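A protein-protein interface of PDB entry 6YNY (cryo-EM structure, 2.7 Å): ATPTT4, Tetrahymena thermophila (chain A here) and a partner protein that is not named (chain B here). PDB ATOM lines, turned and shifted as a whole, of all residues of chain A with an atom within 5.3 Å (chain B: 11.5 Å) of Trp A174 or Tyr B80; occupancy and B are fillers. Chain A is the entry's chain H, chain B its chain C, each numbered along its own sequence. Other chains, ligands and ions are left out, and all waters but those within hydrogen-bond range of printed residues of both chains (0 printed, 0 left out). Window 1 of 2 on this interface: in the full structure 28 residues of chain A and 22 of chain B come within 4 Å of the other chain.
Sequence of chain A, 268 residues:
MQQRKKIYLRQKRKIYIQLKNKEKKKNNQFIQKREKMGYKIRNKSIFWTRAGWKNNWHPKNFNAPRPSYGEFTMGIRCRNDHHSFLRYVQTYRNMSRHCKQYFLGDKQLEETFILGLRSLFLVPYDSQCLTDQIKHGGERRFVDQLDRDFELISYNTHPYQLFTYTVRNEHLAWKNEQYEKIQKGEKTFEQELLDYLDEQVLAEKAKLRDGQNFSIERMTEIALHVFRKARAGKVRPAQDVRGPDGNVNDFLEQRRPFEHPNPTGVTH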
ATOM      1  N   ASN A 169     -15.572  19.323  33.048  1.00  0.00           N
ATOM      2  CA  ASN A 169     -15.888  20.724  33.304  1.00  0.00           C
ATOM      3  C   ASN A 169     -15.040  21.647  32.441  1.00  0.00           C
ATOM      4  O   ASN A 169     -15.529  22.668  31.946  1.00  0.00           O
ATOM      5  CB  ASN A 169     -15.696  21.041  34.783  1.00  0.00           C
ATOM      6  CG  ASN A 169     -16.864  20.595  35.626  1.00  0.00           C
ATOM      7  OD1 ASN A 169     -18.016  20.698  35.214  1.00  0.00           O
ATOM      8  ND2 ASN A 169     -16.572  20.094  36.814  1.00  0.00           N
ATOM      9  N   GLU A 170     -13.763  21.310  32.251  1.00  0.00           N
ATOM     10  CA  GLU A 170     -12.921  22.101  31.364  1.00  0.00           C
ATOM     11  C   GLU A 170     -13.396  22.015  29.922  1.00  0.00           C
ATOM     12  O   GLU A 170     -13.178  22.948  29.141  1.00  0.00           O
ATOM     13  CB  GLU A 170     -11.470  21.641  31.469  1.00  0.00           C
ATOM     14  CG  GLU A 170     -10.840  21.877  32.820  1.00  0.00           C
ATOM     15  CD  GLU A 170      -9.478  21.226  32.957  1.00  0.00           C
ATOM     16  OE1 GLU A 170      -9.059  20.513  32.022  1.00  0.00           O
ATOM     17  OE2 GLU A 170      -8.821  21.431  34.000  1.00  0.00           O
ATOM     18  N   HIS A 171     -14.042  20.910  29.552  1.00  0.00           N
ATOM     19  CA  HIS A 171     -14.529  20.741  28.189  1.00  0.00           C
ATOM     20  C   HIS A 171     -15.833  21.492  27.965  1.00  0.00           C
ATOM     21  O   HIS A 171     -16.001  22.153  26.936  1.00  0.00           O
ATOM     22  CB  HIS A 171     -14.715  19.256  27.892  1.00  0.00           C
ATOM     23  CG  HIS A 171     -15.110  18.963  26.480  1.00  0.00           C
ATOM     24  ND1 HIS A 171     -14.257  19.152  25.415  1.00  0.00           N
ATOM     25  CD2 HIS A 171     -16.265  18.487  25.959  1.00  0.00           C
ATOM     26  CE1 HIS A 171     -14.871  18.809  24.298  1.00  0.00           C
ATOM     27  NE2 HIS A 171     -16.090  18.402  24.600  1.00  0.00           N
ATOM     28  N   LEU A 172     -16.763  21.402  28.916  1.00  0.00           N
ATOM     29  CA  LEU A 172     -18.052  22.060  28.756  1.00  0.00           C
ATOM     30  C   LEU A 172     -17.920  23.572  28.798  1.00  0.00           C
ATOM     31  O   LEU A 172     -18.675  24.280  28.122  1.00  0.00           O
ATOM     32  CB  LEU A 172     -19.014  21.583  29.838  1.00  0.00           C
ATOM     33  CG  LEU A 172     -19.307  20.088  29.820  1.00  0.00           C
ATOM     34  CD1 LEU A 172     -20.125  19.696  31.019  1.00  0.00           C
ATOM     35  CD2 LEU A 172     -20.022  19.713  28.546  1.00  0.00           C
ATOM     36  N   ALA A 173     -16.976  24.085  29.584  1.00  0.00           N
ATOM     37  CA  ALA A 173     -16.751  25.522  29.620  1.00  0.00           C
ATOM     38  C   ALA A 173     -16.336  26.050  28.257  1.00  0.00           C
ATOM     39  O   ALA A 173     -16.696  27.172  27.887  1.00  0.00           O
ATOM     40  CB  ALA A 173     -15.687  25.851  30.660  1.00  0.00           C
ATOM     41  N   TRP A 174     -15.580  25.257  27.500  1.00  0.00           N
ATOM     42  CA  TRP A 174     -15.136  25.674  26.179  1.00  0.00           C
ATOM     43  C   TRP A 174     -16.230  25.502  25.137  1.00  0.00           C
ATOM     44  O   TRP A 174     -16.288  26.271  24.173  1.00  0.00           O
ATOM     45  CB  TRP A 174     -13.887  24.887  25.791  1.00  0.00           C
ATOM     46  CG  TRP A 174     -13.388  25.155  24.418  1.00  0.00           C
ATOM     47  CD1 TRP A 174     -13.064  26.364  23.885  1.00  0.00           C
ATOM     48  CD2 TRP A 174     -13.128  24.186  23.399  1.00  0.00           C
ATOM     49  NE1 TRP A 174     -12.627  26.211  22.594  1.00  0.00           N
ATOM     50  CE2 TRP A 174     -12.656  24.881  22.272  1.00  0.00           C
ATOM     51  CE3 TRP A 174     -13.251  22.797  23.330  1.00  0.00           C
ATOM     52  CZ2 TRP A 174     -12.311  24.237  21.092  1.00  0.00           C
ATOM     53  CZ3 TRP A 174     -12.908  22.160  22.158  1.00  0.00           C
ATOM     54  CH2 TRP A 174     -12.443  22.879  21.054  1.00  0.00           C
ATOM     55  N   LYS A 175     -17.102  24.507  25.311  1.00  0.00           N
ATOM     56  CA  LYS A 175     -18.232  24.353  24.405  1.00  0.00           C
ATOM     57  C   LYS A 175     -19.298  25.409  24.656  1.00  0.00           C
ATOM     58  O   LYS A 175     -19.989  25.824  23.721  1.00  0.00           O
ATOM     59  CB  LYS A 175     -18.827  22.954  24.543  1.00  0.00           C
ATOM     60  CG  LYS A 175     -18.044  21.881  23.820  1.00  0.00           C
ATOM     61  CD  LYS A 175     -18.289  21.928  22.326  1.00  0.00           C
ATOM     62  CE  LYS A 175     -17.410  20.942  21.585  1.00  0.00           C
ATOM     63  NZ  LYS A 175     -15.972  21.313  21.676  1.00  0.00           N
ATOM     64  N   ASN A 176     -19.452  25.849  25.905  1.00  0.00           N
ATOM     65  CA  ASN A 176     -20.392  26.924  26.196  1.00  0.00           C
ATOM     66  C   ASN A 176     -19.872  28.265  25.702  1.00  0.00           C
ATOM     67  O   ASN A 176     -20.663  29.123  25.294  1.00  0.00           O
ATOM     68  CB  ASN A 176     -20.674  26.980  27.693  1.00  0.00           C
ATOM     69  CG  ASN A 176     -21.725  25.983  28.120  1.00  0.00           C
ATOM     70  OD1 ASN A 176     -22.752  25.829  27.462  1.00  0.00           O
ATOM     71  ND2 ASN A 176     -21.473  25.295  29.223  1.00  0.00           N
ATOM     72  N   GLU A 177     -18.555  28.465  25.730  1.00  0.00           N
ATOM     73  CA  GLU A 177     -17.984  29.689  25.183  1.00  0.00           C
ATOM     74  C   GLU A 177     -18.250  29.787  23.688  1.00  0.00           C
ATOM     75  O   GLU A 177     -18.477  30.881  23.159  1.00  0.00           O
ATOM     76  CB  GLU A 177     -16.486  29.739  25.472  1.00  0.00           C
ATOM     77  CG  GLU A 177     -15.786  30.968  24.929  1.00  0.00           C
ATOM     78  CD  GLU A 177     -14.319  31.013  25.304  1.00  0.00           C
ATOM     79  OE1 GLU A 177     -13.857  30.090  26.005  1.00  0.00           O
ATOM     80  OE2 GLU A 177     -13.631  31.971  24.896  1.00  0.00           O
ATOM     81  N   GLN A 178     -18.221  28.651  22.989  1.00  0.00           N
ATOM     82  CA  GLN A 178     -18.545  28.647  21.569  1.00  0.00           C
ATOM     83  C   GLN A 178     -20.027  28.907  21.341  1.00  0.00           C
ATOM     84  O   GLN A 178     -20.401  29.648  20.426  1.00  0.00           O
ATOM     85  CB  GLN A 178     -18.139  27.316  20.946  1.00  0.00           C
ATOM     86  CG  GLN A 178     -16.650  27.069  20.925  1.00  0.00           C
ATOM     87  CD  GLN A 178     -16.295  25.761  20.257  1.00  0.00           C
ATOM     88  OE1 GLN A 178     -16.889  24.722  20.542  1.00  0.00           O
ATOM     89  NE2 GLN A 178     -15.328  25.805  19.350  1.00  0.00           N
ATOM     90  N   GLU A 190     -12.301  28.722  16.048  1.00  0.00           N
ATOM     91  CA  GLU A 190     -12.104  27.486  15.304  1.00  0.00           C
ATOM     92  C   GLU A 190     -12.615  27.604  13.877  1.00  0.00           C
ATOM     93  O   GLU A 190     -12.054  26.981  12.970  1.00  0.00           O
ATOM     94  CB  GLU A 190     -12.797  26.327  16.021  1.00  0.00           C
ATOM     95  CG  GLU A 190     -12.199  25.976  17.376  1.00  0.00           C
ATOM     96  CD  GLU A 190     -12.516  26.996  18.450  1.00  0.00           C
ATOM     97  OE1 GLU A 190     -13.321  27.911  18.185  1.00  0.00           O
ATOM     98  OE2 GLU A 190     -11.961  26.885  19.562  1.00  0.00           O
ATOM     99  N   ARG B  68      -4.965   1.553  24.676  1.00  0.00           N
ATOM    100  CA  ARG B  68      -5.278   2.814  25.325  1.00  0.00           C
ATOM    101  C   ARG B  68      -5.820   2.577  26.729  1.00  0.00           C
ATOM    102  O   ARG B  68      -6.574   1.632  26.971  1.00  0.00           O
ATOM    103  CB  ARG B  68      -6.292   3.580  24.484  1.00  0.00           C
ATOM    104  CG  ARG B  68      -6.429   5.037  24.823  1.00  0.00           C
ATOM    105  CD  ARG B  68      -7.390   5.717  23.878  1.00  0.00           C
ATOM    106  NE  ARG B  68      -6.906   5.713  22.502  1.00  0.00           N
ATOM    107  CZ  ARG B  68      -6.172   6.675  21.955  1.00  0.00           C
ATOM    108  NH1 ARG B  68      -5.824   7.741  22.656  1.00  0.00           N
ATOM    109  NH2 ARG B  68      -5.785   6.571  20.694  1.00  0.00           N
ATOM    110  N   THR B  71      -7.328   6.998  31.132  1.00  0.00           N
ATOM    111  CA  THR B  71      -6.984   8.409  31.027  1.00  0.00           C
ATOM    112  C   THR B  71      -6.806   8.831  29.576  1.00  0.00           C
ATOM    113  O   THR B  71      -7.256   9.909  29.176  1.00  0.00           O
ATOM    114  CB  THR B  71      -5.715   8.689  31.823  1.00  0.00           C
ATOM    115  OG1 THR B  71      -4.684   7.786  31.410  1.00  0.00           O
ATOM    116  CG2 THR B  71      -5.973   8.515  33.295  1.00  0.00           C
ATOM    117  N   GLU B  72      -6.153   7.994  28.774  1.00  0.00           N
ATOM    118  CA  GLU B  72      -5.952   8.315  27.370  1.00  0.00           C
ATOM    119  C   GLU B  72      -7.260   8.331  26.591  1.00  0.00           C
ATOM    120  O   GLU B  72      -7.323   8.947  25.523  1.00  0.00           O
ATOM    121  CB  GLU B  72      -4.975   7.317  26.756  1.00  0.00           C
ATOM    122  CG  GLU B  72      -3.584   7.383  27.361  1.00  0.00           C
ATOM    123  CD  GLU B  72      -2.726   6.187  27.004  1.00  0.00           C
ATOM    124  OE1 GLU B  72      -3.258   5.221  26.421  1.00  0.00           O
ATOM    125  OE2 GLU B  72      -1.517   6.212  27.311  1.00  0.00           O
ATOM    126  N   VAL B  73      -8.300   7.676  27.100  1.00  0.00           N
ATOM    127  CA  VAL B  73      -9.603   7.722  26.448  1.00  0.00           C
ATOM    128  C   VAL B  73     -10.298   9.044  26.736  1.00  0.00           C
ATOM    129  O   VAL B  73     -10.826   9.695  25.828  1.00  0.00           O
ATOM    130  CB  VAL B  73     -10.466   6.530  26.897  1.00  0.00           C
ATOM    131  CG1 VAL B  73     -11.871   6.677  26.367  1.00  0.00           C
ATOM    132  CG2 VAL B  73      -9.869   5.230  26.429  1.00  0.00           C
ATOM    133  N   LEU B  74     -10.318   9.454  28.003  1.00  0.00           N
ATOM    134  CA  LEU B  74     -10.973  10.706  28.363  1.00  0.00           C
ATOM    135  C   LEU B  74     -10.245  11.904  27.771  1.00  0.00           C
ATOM    136  O   LEU B  74     -10.881  12.859  27.312  1.00  0.00           O
ATOM    137  CB  LEU B  74     -11.055  10.832  29.883  1.00  0.00           C
ATOM    138  CG  LEU B  74     -12.222  10.141  30.579  1.00  0.00           C
ATOM    139  CD1 LEU B  74     -13.522  10.828  30.227  1.00  0.00           C
ATOM    140  CD2 LEU B  74     -12.282   8.675  30.223  1.00  0.00           C
ATOM    141  N   LEU B  75      -8.914  11.871  27.766  1.00  0.00           N
ATOM    142  CA  LEU B  75      -8.151  12.995  27.244  1.00  0.00           C
ATOM    143  C   LEU B  75      -8.371  13.171  25.749  1.00  0.00           C
ATOM    144  O   LEU B  75      -8.415  14.301  25.251  1.00  0.00           O
ATOM    145  CB  LEU B  75      -6.669  12.797  27.541  1.00  0.00           C
ATOM    146  CG  LEU B  75      -6.252  12.896  29.004  1.00  0.00           C
ATOM    147  CD1 LEU B  75      -4.814  12.463  29.173  1.00  0.00           C
ATOM    148  CD2 LEU B  75      -6.443  14.300  29.515  1.00  0.00           C
ATOM    149  N   LYS B  76      -8.514  12.067  25.020  1.00  0.00           N
ATOM    150  CA  LYS B  76      -8.691  12.151  23.577  1.00  0.00           C
ATOM    151  C   LYS B  76     -10.072  12.665  23.202  1.00  0.00           C
ATOM    152  O   LYS B  76     -10.217  13.366  22.195  1.00  0.00           O
ATOM    153  CB  LYS B  76      -8.453  10.779  22.953  1.00  0.00           C
ATOM    154  CG  LYS B  76      -8.695  10.704  21.467  1.00  0.00           C
ATOM    155  CD  LYS B  76      -8.592   9.288  20.984  1.00  0.00           C
ATOM    156  CE  LYS B  76      -8.927   9.182  19.518  1.00  0.00           C
ATOM    157  NZ  LYS B  76      -7.947   9.918  18.705  1.00  0.00           N
ATOM    158  N   ILE B  77     -11.089  12.338  23.992  1.00  0.00           N
ATOM    159  CA  ILE B  77     -12.472  12.592  23.615  1.00  0.00           C
ATOM    160  C   ILE B  77     -13.011  13.831  24.314  1.00  0.00           C
ATOM    161  O   ILE B  77     -13.857  14.542  23.762  1.00  0.00           O
ATOM    162  CB  ILE B  77     -13.344  11.366  23.925  1.00  0.00           C
ATOM    163  CG1 ILE B  77     -12.985  10.221  22.983  1.00  0.00           C
ATOM    164  CG2 ILE B  77     -14.808  11.721  23.809  1.00  0.00           C
ATOM    165  CD1 ILE B  77     -13.477   8.895  23.438  1.00  0.00           C
ATOM    166  N   SER B  78     -12.536  14.098  25.529  1.00  0.00           N
ATOM    167  CA  SER B  78     -13.068  15.191  26.331  1.00  0.00           C
ATOM    168  C   SER B  78     -12.002  16.188  26.764  1.00  0.00           C
ATOM    169  O   SER B  78     -12.273  17.021  27.634  1.00  0.00           O
ATOM    170  CB  SER B  78     -13.785  14.637  27.560  1.00  0.00           C
ATOM    171  OG  SER B  78     -14.431  15.670  28.275  1.00  0.00           O
ATOM    172  N   ALA B  79     -10.799  16.126  26.193  1.00  0.00           N
ATOM    173  CA  ALA B  79      -9.766  17.091  26.545  1.00  0.00           C
ATOM    174  C   ALA B  79      -8.960  17.535  25.332  1.00  0.00           C
ATOM    175  O   ALA B  79      -7.829  18.004  25.491  1.00  0.00           O
ATOM    176  CB  ALA B  79      -8.820  16.525  27.596  1.00  0.00           C
ATOM    177  N   TYR B  80      -9.507  17.403  24.131  1.00  0.00           N
ATOM    178  CA  TYR B  80      -8.813  17.859  22.940  1.00  0.00           C
ATOM    179  C   TYR B  80      -8.866  19.377  22.840  1.00  0.00           C
ATOM    180  O   TYR B  80      -9.802  20.023  23.316  1.00  0.00           O
ATOM    181  CB  TYR B  80      -9.413  17.228  21.685  1.00  0.00           C
ATOM    182  CG  TYR B  80     -10.881  17.504  21.476  1.00  0.00           C
ATOM    183  CD1 TYR B  80     -11.306  18.662  20.851  1.00  0.00           C
ATOM    184  CD2 TYR B  80     -11.839  16.597  21.887  1.00  0.00           C
ATOM    185  CE1 TYR B  80     -12.640  18.914  20.655  1.00  0.00           C
ATOM    186  CE2 TYR B  80     -13.175  16.841  21.693  1.00  0.00           C
ATOM    187  CZ  TYR B  80     -13.571  18.000  21.076  1.00  0.00           C
ATOM    188  OH  TYR B  80     -14.907  18.242  20.883  1.00  0.00           O
ATOM    189  N   ASN B  81      -7.838  19.942  22.220  1.00  0.00           N
ATOM    190  CA  ASN B  81      -7.705  21.383  22.107  1.00  0.00           C
ATOM    191  C   ASN B  81      -8.365  21.858  20.815  1.00  0.00           C
ATOM    192  O   ASN B  81      -9.032  21.097  20.110  1.00  0.00           O
ATOM    193  CB  ASN B  81      -6.234  21.784  22.178  1.00  0.00           C
ATOM    194  CG  ASN B  81      -5.404  21.149  21.091  1.00  0.00           C
ATOM    195  OD1 ASN B  81      -5.925  20.455  20.222  1.00  0.00           O
ATOM    196  ND2 ASN B  81      -4.104  21.390  21.128  1.00  0.00           N
ATOM    197  N   ASP B  82      -8.180  23.136  20.489  1.00  0.00           N
ATOM    198  CA  ASP B  82      -8.818  23.711  19.312  1.00  0.00           C
ATOM    199  C   ASP B  82      -8.139  23.265  18.024  1.00  0.00           C
ATOM    200  O   ASP B  82      -8.816  22.972  17.034  1.00  0.00           O
ATOM    201  CB  ASP B  82      -8.814  25.234  19.417  1.00  0.00           C
ATOM    202  CG  ASP B  82      -7.438  25.795  19.692  1.00  0.00           C
ATOM    203  OD1 ASP B  82      -6.483  25.000  19.808  1.00  0.00           O
ATOM    204  OD2 ASP B  82      -7.309  27.031  19.802  1.00  0.00           O
ATOM    205  N   PHE B  83      -6.806  23.214  18.012  1.00  0.00           N
ATOM    206  CA  PHE B  83      -6.100  22.809  16.804  1.00  0.00           C
ATOM    207  C   PHE B  83      -6.471  21.390  16.396  1.00  0.00           C
ATOM    208  O   PHE B  83      -6.576  21.086  15.203  1.00  0.00           O
ATOM    209  CB  PHE B  83      -4.593  22.928  17.012  1.00  0.00           C
ATOM    210  CG  PHE B  83      -4.118  24.329  17.261  1.00  0.00           C
ATOM    211  CD1 PHE B  83      -4.823  25.416  16.784  1.00  0.00           C
ATOM    212  CD2 PHE B  83      -2.959  24.557  17.971  1.00  0.00           C
ATOM    213  CE1 PHE B  83      -4.382  26.695  17.013  1.00  0.00           C
ATOM    214  CE2 PHE B  83      -2.515  25.836  18.203  1.00  0.00           C
ATOM    215  CZ  PHE B  83      -3.227  26.906  17.722  1.00  0.00           C
ATOM    216  N   PHE B  84      -6.676  20.508  17.372  1.00  0.00           N
ATOM    217  CA  PHE B  84      -7.075  19.142  17.059  1.00  0.00           C
ATOM    218  C   PHE B  84      -8.467  19.106  16.447  1.00  0.00           C
ATOM    219  O   PHE B  84      -8.715  18.359  15.494  1.00  0.00           O
ATOM    220  CB  PHE B  84      -7.017  18.283  18.318  1.00  0.00           C
ATOM    221  CG  PHE B  84      -7.366  16.849  18.087  1.00  0.00           C
ATOM    222  CD1 PHE B  84      -8.632  16.380  18.362  1.00  0.00           C
ATOM    223  CD2 PHE B  84      -6.429  15.971  17.590  1.00  0.00           C
ATOM    224  CE1 PHE B  84      -8.953  15.063  18.149  1.00  0.00           C
ATOM    225  CE2 PHE B  84      -6.744  14.656  17.374  1.00  0.00           C
ATOM    226  CZ  PHE B  84      -8.007  14.199  17.655  1.00  0.00           C
ATOM    227  N   TYR B  85      -9.389  19.905  16.983  1.00  0.00           N
ATOM    228  CA  TYR B  85     -10.722  19.993  16.403  1.00  0.00           C
ATOM    229  C   TYR B  85     -10.664  20.538  14.985  1.00  0.00           C
ATOM    230  O   TYR B  85     -11.377  20.060  14.095  1.00  0.00           O
ATOM    231  CB  TYR B  85     -11.603  20.874  17.282  1.00  0.00           C
ATOM    232  CG  TYR B  85     -13.024  21.021  16.802  1.00  0.00           C
ATOM    233  CD1 TYR B  85     -13.973  20.053  17.082  1.00  0.00           C
ATOM    234  CD2 TYR B  85     -13.419  22.133  16.081  1.00  0.00           C
ATOM    235  CE1 TYR B  85     -15.270  20.185  16.652  1.00  0.00           C
ATOM    236  CE2 TYR B  85     -14.716  22.273  15.644  1.00  0.00           C
ATOM    237  CZ  TYR B  85     -15.638  21.296  15.934  1.00  0.00           C
ATOM    238  OH  TYR B  85     -16.935  21.432  15.501  1.00  0.00           O
ATOM    239  N   VAL B  86      -9.816  21.538  14.755  1.00  0.00           N
ATOM    240  CA  VAL B  86      -9.705  22.138  13.433  1.00  0.00           C
ATOM    241  C   VAL B  86      -9.117  21.145  12.443  1.00  0.00           C
ATOM    242  O   VAL B  86      -9.604  21.008  11.315  1.00  0.00           O
ATOM    243  CB  VAL B  86      -8.864  23.422  13.514  1.00  0.00           C
ATOM    244  CG1 VAL B  86      -8.504  23.915  12.133  1.00  0.00           C
ATOM    245  CG2 VAL B  86      -9.609  24.484  14.282  1.00  0.00           C
ATOM    246  N   LEU B  87      -8.062  20.439  12.845  1.00  0.00           N
ATOM    247  CA  LEU B  87      -7.381  19.539  11.926  1.00  0.00           C
ATOM    248  C   LEU B  87      -8.296  18.409  11.476  1.00  0.00           C
ATOM    249  O   LEU B  87      -8.275  18.012  10.307  1.00  0.00           O
ATOM    250  CB  LEU B  87      -6.124  18.985  12.588  1.00  0.00           C
ATOM    251  CG  LEU B  87      -5.134  18.271  11.678  1.00  0.00           C
ATOM    252  CD1 LEU B  87      -4.490  19.250  10.725  1.00  0.00           C
ATOM    253  CD2 LEU B  87      -4.095  17.571  12.506  1.00  0.00           C
ATOM    254  N   ASN B  88      -9.109  17.877  12.389  1.00  0.00           N
ATOM    255  CA  ASN B  88     -10.027  16.804  12.025  1.00  0.00           C
ATOM    256  C   ASN B  88     -11.059  17.285  11.015  1.00  0.00           C
ATOM    257  O   ASN B  88     -11.242  16.672   9.958  1.00  0.00           O
ATOM    258  CB  ASN B  88     -10.712  16.253  13.274  1.00  0.00           C
ATOM    259  CG  ASN B  88      -9.847  15.279  14.031  1.00  0.00           C
ATOM    260  OD1 ASN B  88      -9.944  14.067  13.842  1.00  0.00           O
ATOM    261  ND2 ASN B  88      -8.994  15.800  14.899  1.00  0.00           N
ATOM    262  N   ASN B  89     -11.753  18.381  11.326  1.00  0.00           N
ATOM    263  CA  ASN B  89     -12.741  18.909  10.393  1.00  0.00           C
ATOM    264  C   ASN B  89     -12.088  19.427   9.121  1.00  0.00           C
ATOM    265  O   ASN B  89     -12.693  19.368   8.047  1.00  0.00           O
ATOM    266  CB  ASN B  89     -13.550  20.015  11.060  1.00  0.00           C
ATOM    267  CG  ASN B  89     -14.396  19.506  12.200  1.00  0.00           C
ATOM    268  OD1 ASN B  89     -15.576  19.207  12.030  1.00  0.00           O
ATOM    269  ND2 ASN B  89     -13.795  19.398  13.373  1.00  0.00           N
ATOM    270  N   TYR B  92     -11.718  16.404   7.096  1.00  0.00           N
ATOM    271  CA  TYR B  92     -13.012  15.889   6.668  1.00  0.00           C
ATOM    272  C   TYR B  92     -13.589  16.723   5.533  1.00  0.00           C
ATOM    273  O   TYR B  92     -13.979  16.186   4.491  1.00  0.00           O
ATOM    274  CB  TYR B  92     -13.983  15.861   7.845  1.00  0.00           C
ATOM    275  CG  TYR B  92     -13.672  14.840   8.912  1.00  0.00           C
ATOM    276  CD1 TYR B  92     -12.519  14.075   8.865  1.00  0.00           C
ATOM    277  CD2 TYR B  92     -14.544  14.637   9.966  1.00  0.00           C
ATOM    278  CE1 TYR B  92     -12.245  13.146   9.839  1.00  0.00           C
ATOM    279  CE2 TYR B  92     -14.277  13.710  10.941  1.00  0.00           C
ATOM    280  CZ  TYR B  92     -13.129  12.968  10.874  1.00  0.00           C
ATOM    281  OH  TYR B  92     -12.865  12.042  11.850  1.00  0.00           O
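OH of Tyr B80 lies within hydrogen-bond range of NZ of Lys A175 (3.3 Å).
The backbone carbonyl oxygen (O) of Leu B75 is in hydrogen-bond range of the backbone NH (N) of Tyr B80 (3.5 Å). OD1 of Asn B81 sits at hydrogen-bond distance from N of Phe B84. NE1 of Trp A174 lies close to OE2 of Glu A190 (3.2 Å). NE2 of Gln A178 is in hydrogen-bond range of OE1 of Glu A190, 3.1 Å away.
Among the printed residues, merely in contact across the chains: His A171 with Ser B78, His A171 with Tyr B80, Glu A190 with Asp B82, Trp A174 with Tyr B80, Glu A190 with Val B86, Trp A174 with Asp B82 and Trp A174 with Asn B81.
No residue of chain B comes within 4 Å of Ala A173. Trp A174 touches three residues of chain B. No residue of chain B comes within 4 Å of Asn A176. No residue of chain B comes within 4 Å of Glu A177. Gln A178 touches none of the printed residues of chain B. Printed residues of chain A within 4 Å of Ser B78: His A171 (3.3 Å). Of chain A, only His A171 (3.5 Å), Trp A174 (3.6 Å) and Lys A175 (3.3 Å) come within 4 Å of Tyr B80. Of the printed residues of chain A, Asn B81 touches Trp A174 (3.96 Å). Of the printed residues of chain A, Asp B82 touches Trp A174 (3.96 Å) and Glu A190 (3.6 Å). Of the printed residues of chain A, Val B86 touches Glu A190 (3.7 Å). The nearest residue of chain B that does not touch Trp A174 is Tyr B85 (4.4 Å). The nearest printed residue of chain A that does not touch Tyr B80 is Gln A178 (6.8 Å).
Of the 21 printed residues of chain B, 5 touch a printed residue of chain A. Among the printed residues, 8 pairs touch across the chains. Among the printed residues, no Asp or Glu carboxylate lies within 4 Å of a Lys or Arg side-chain nitrogen of the other chain.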
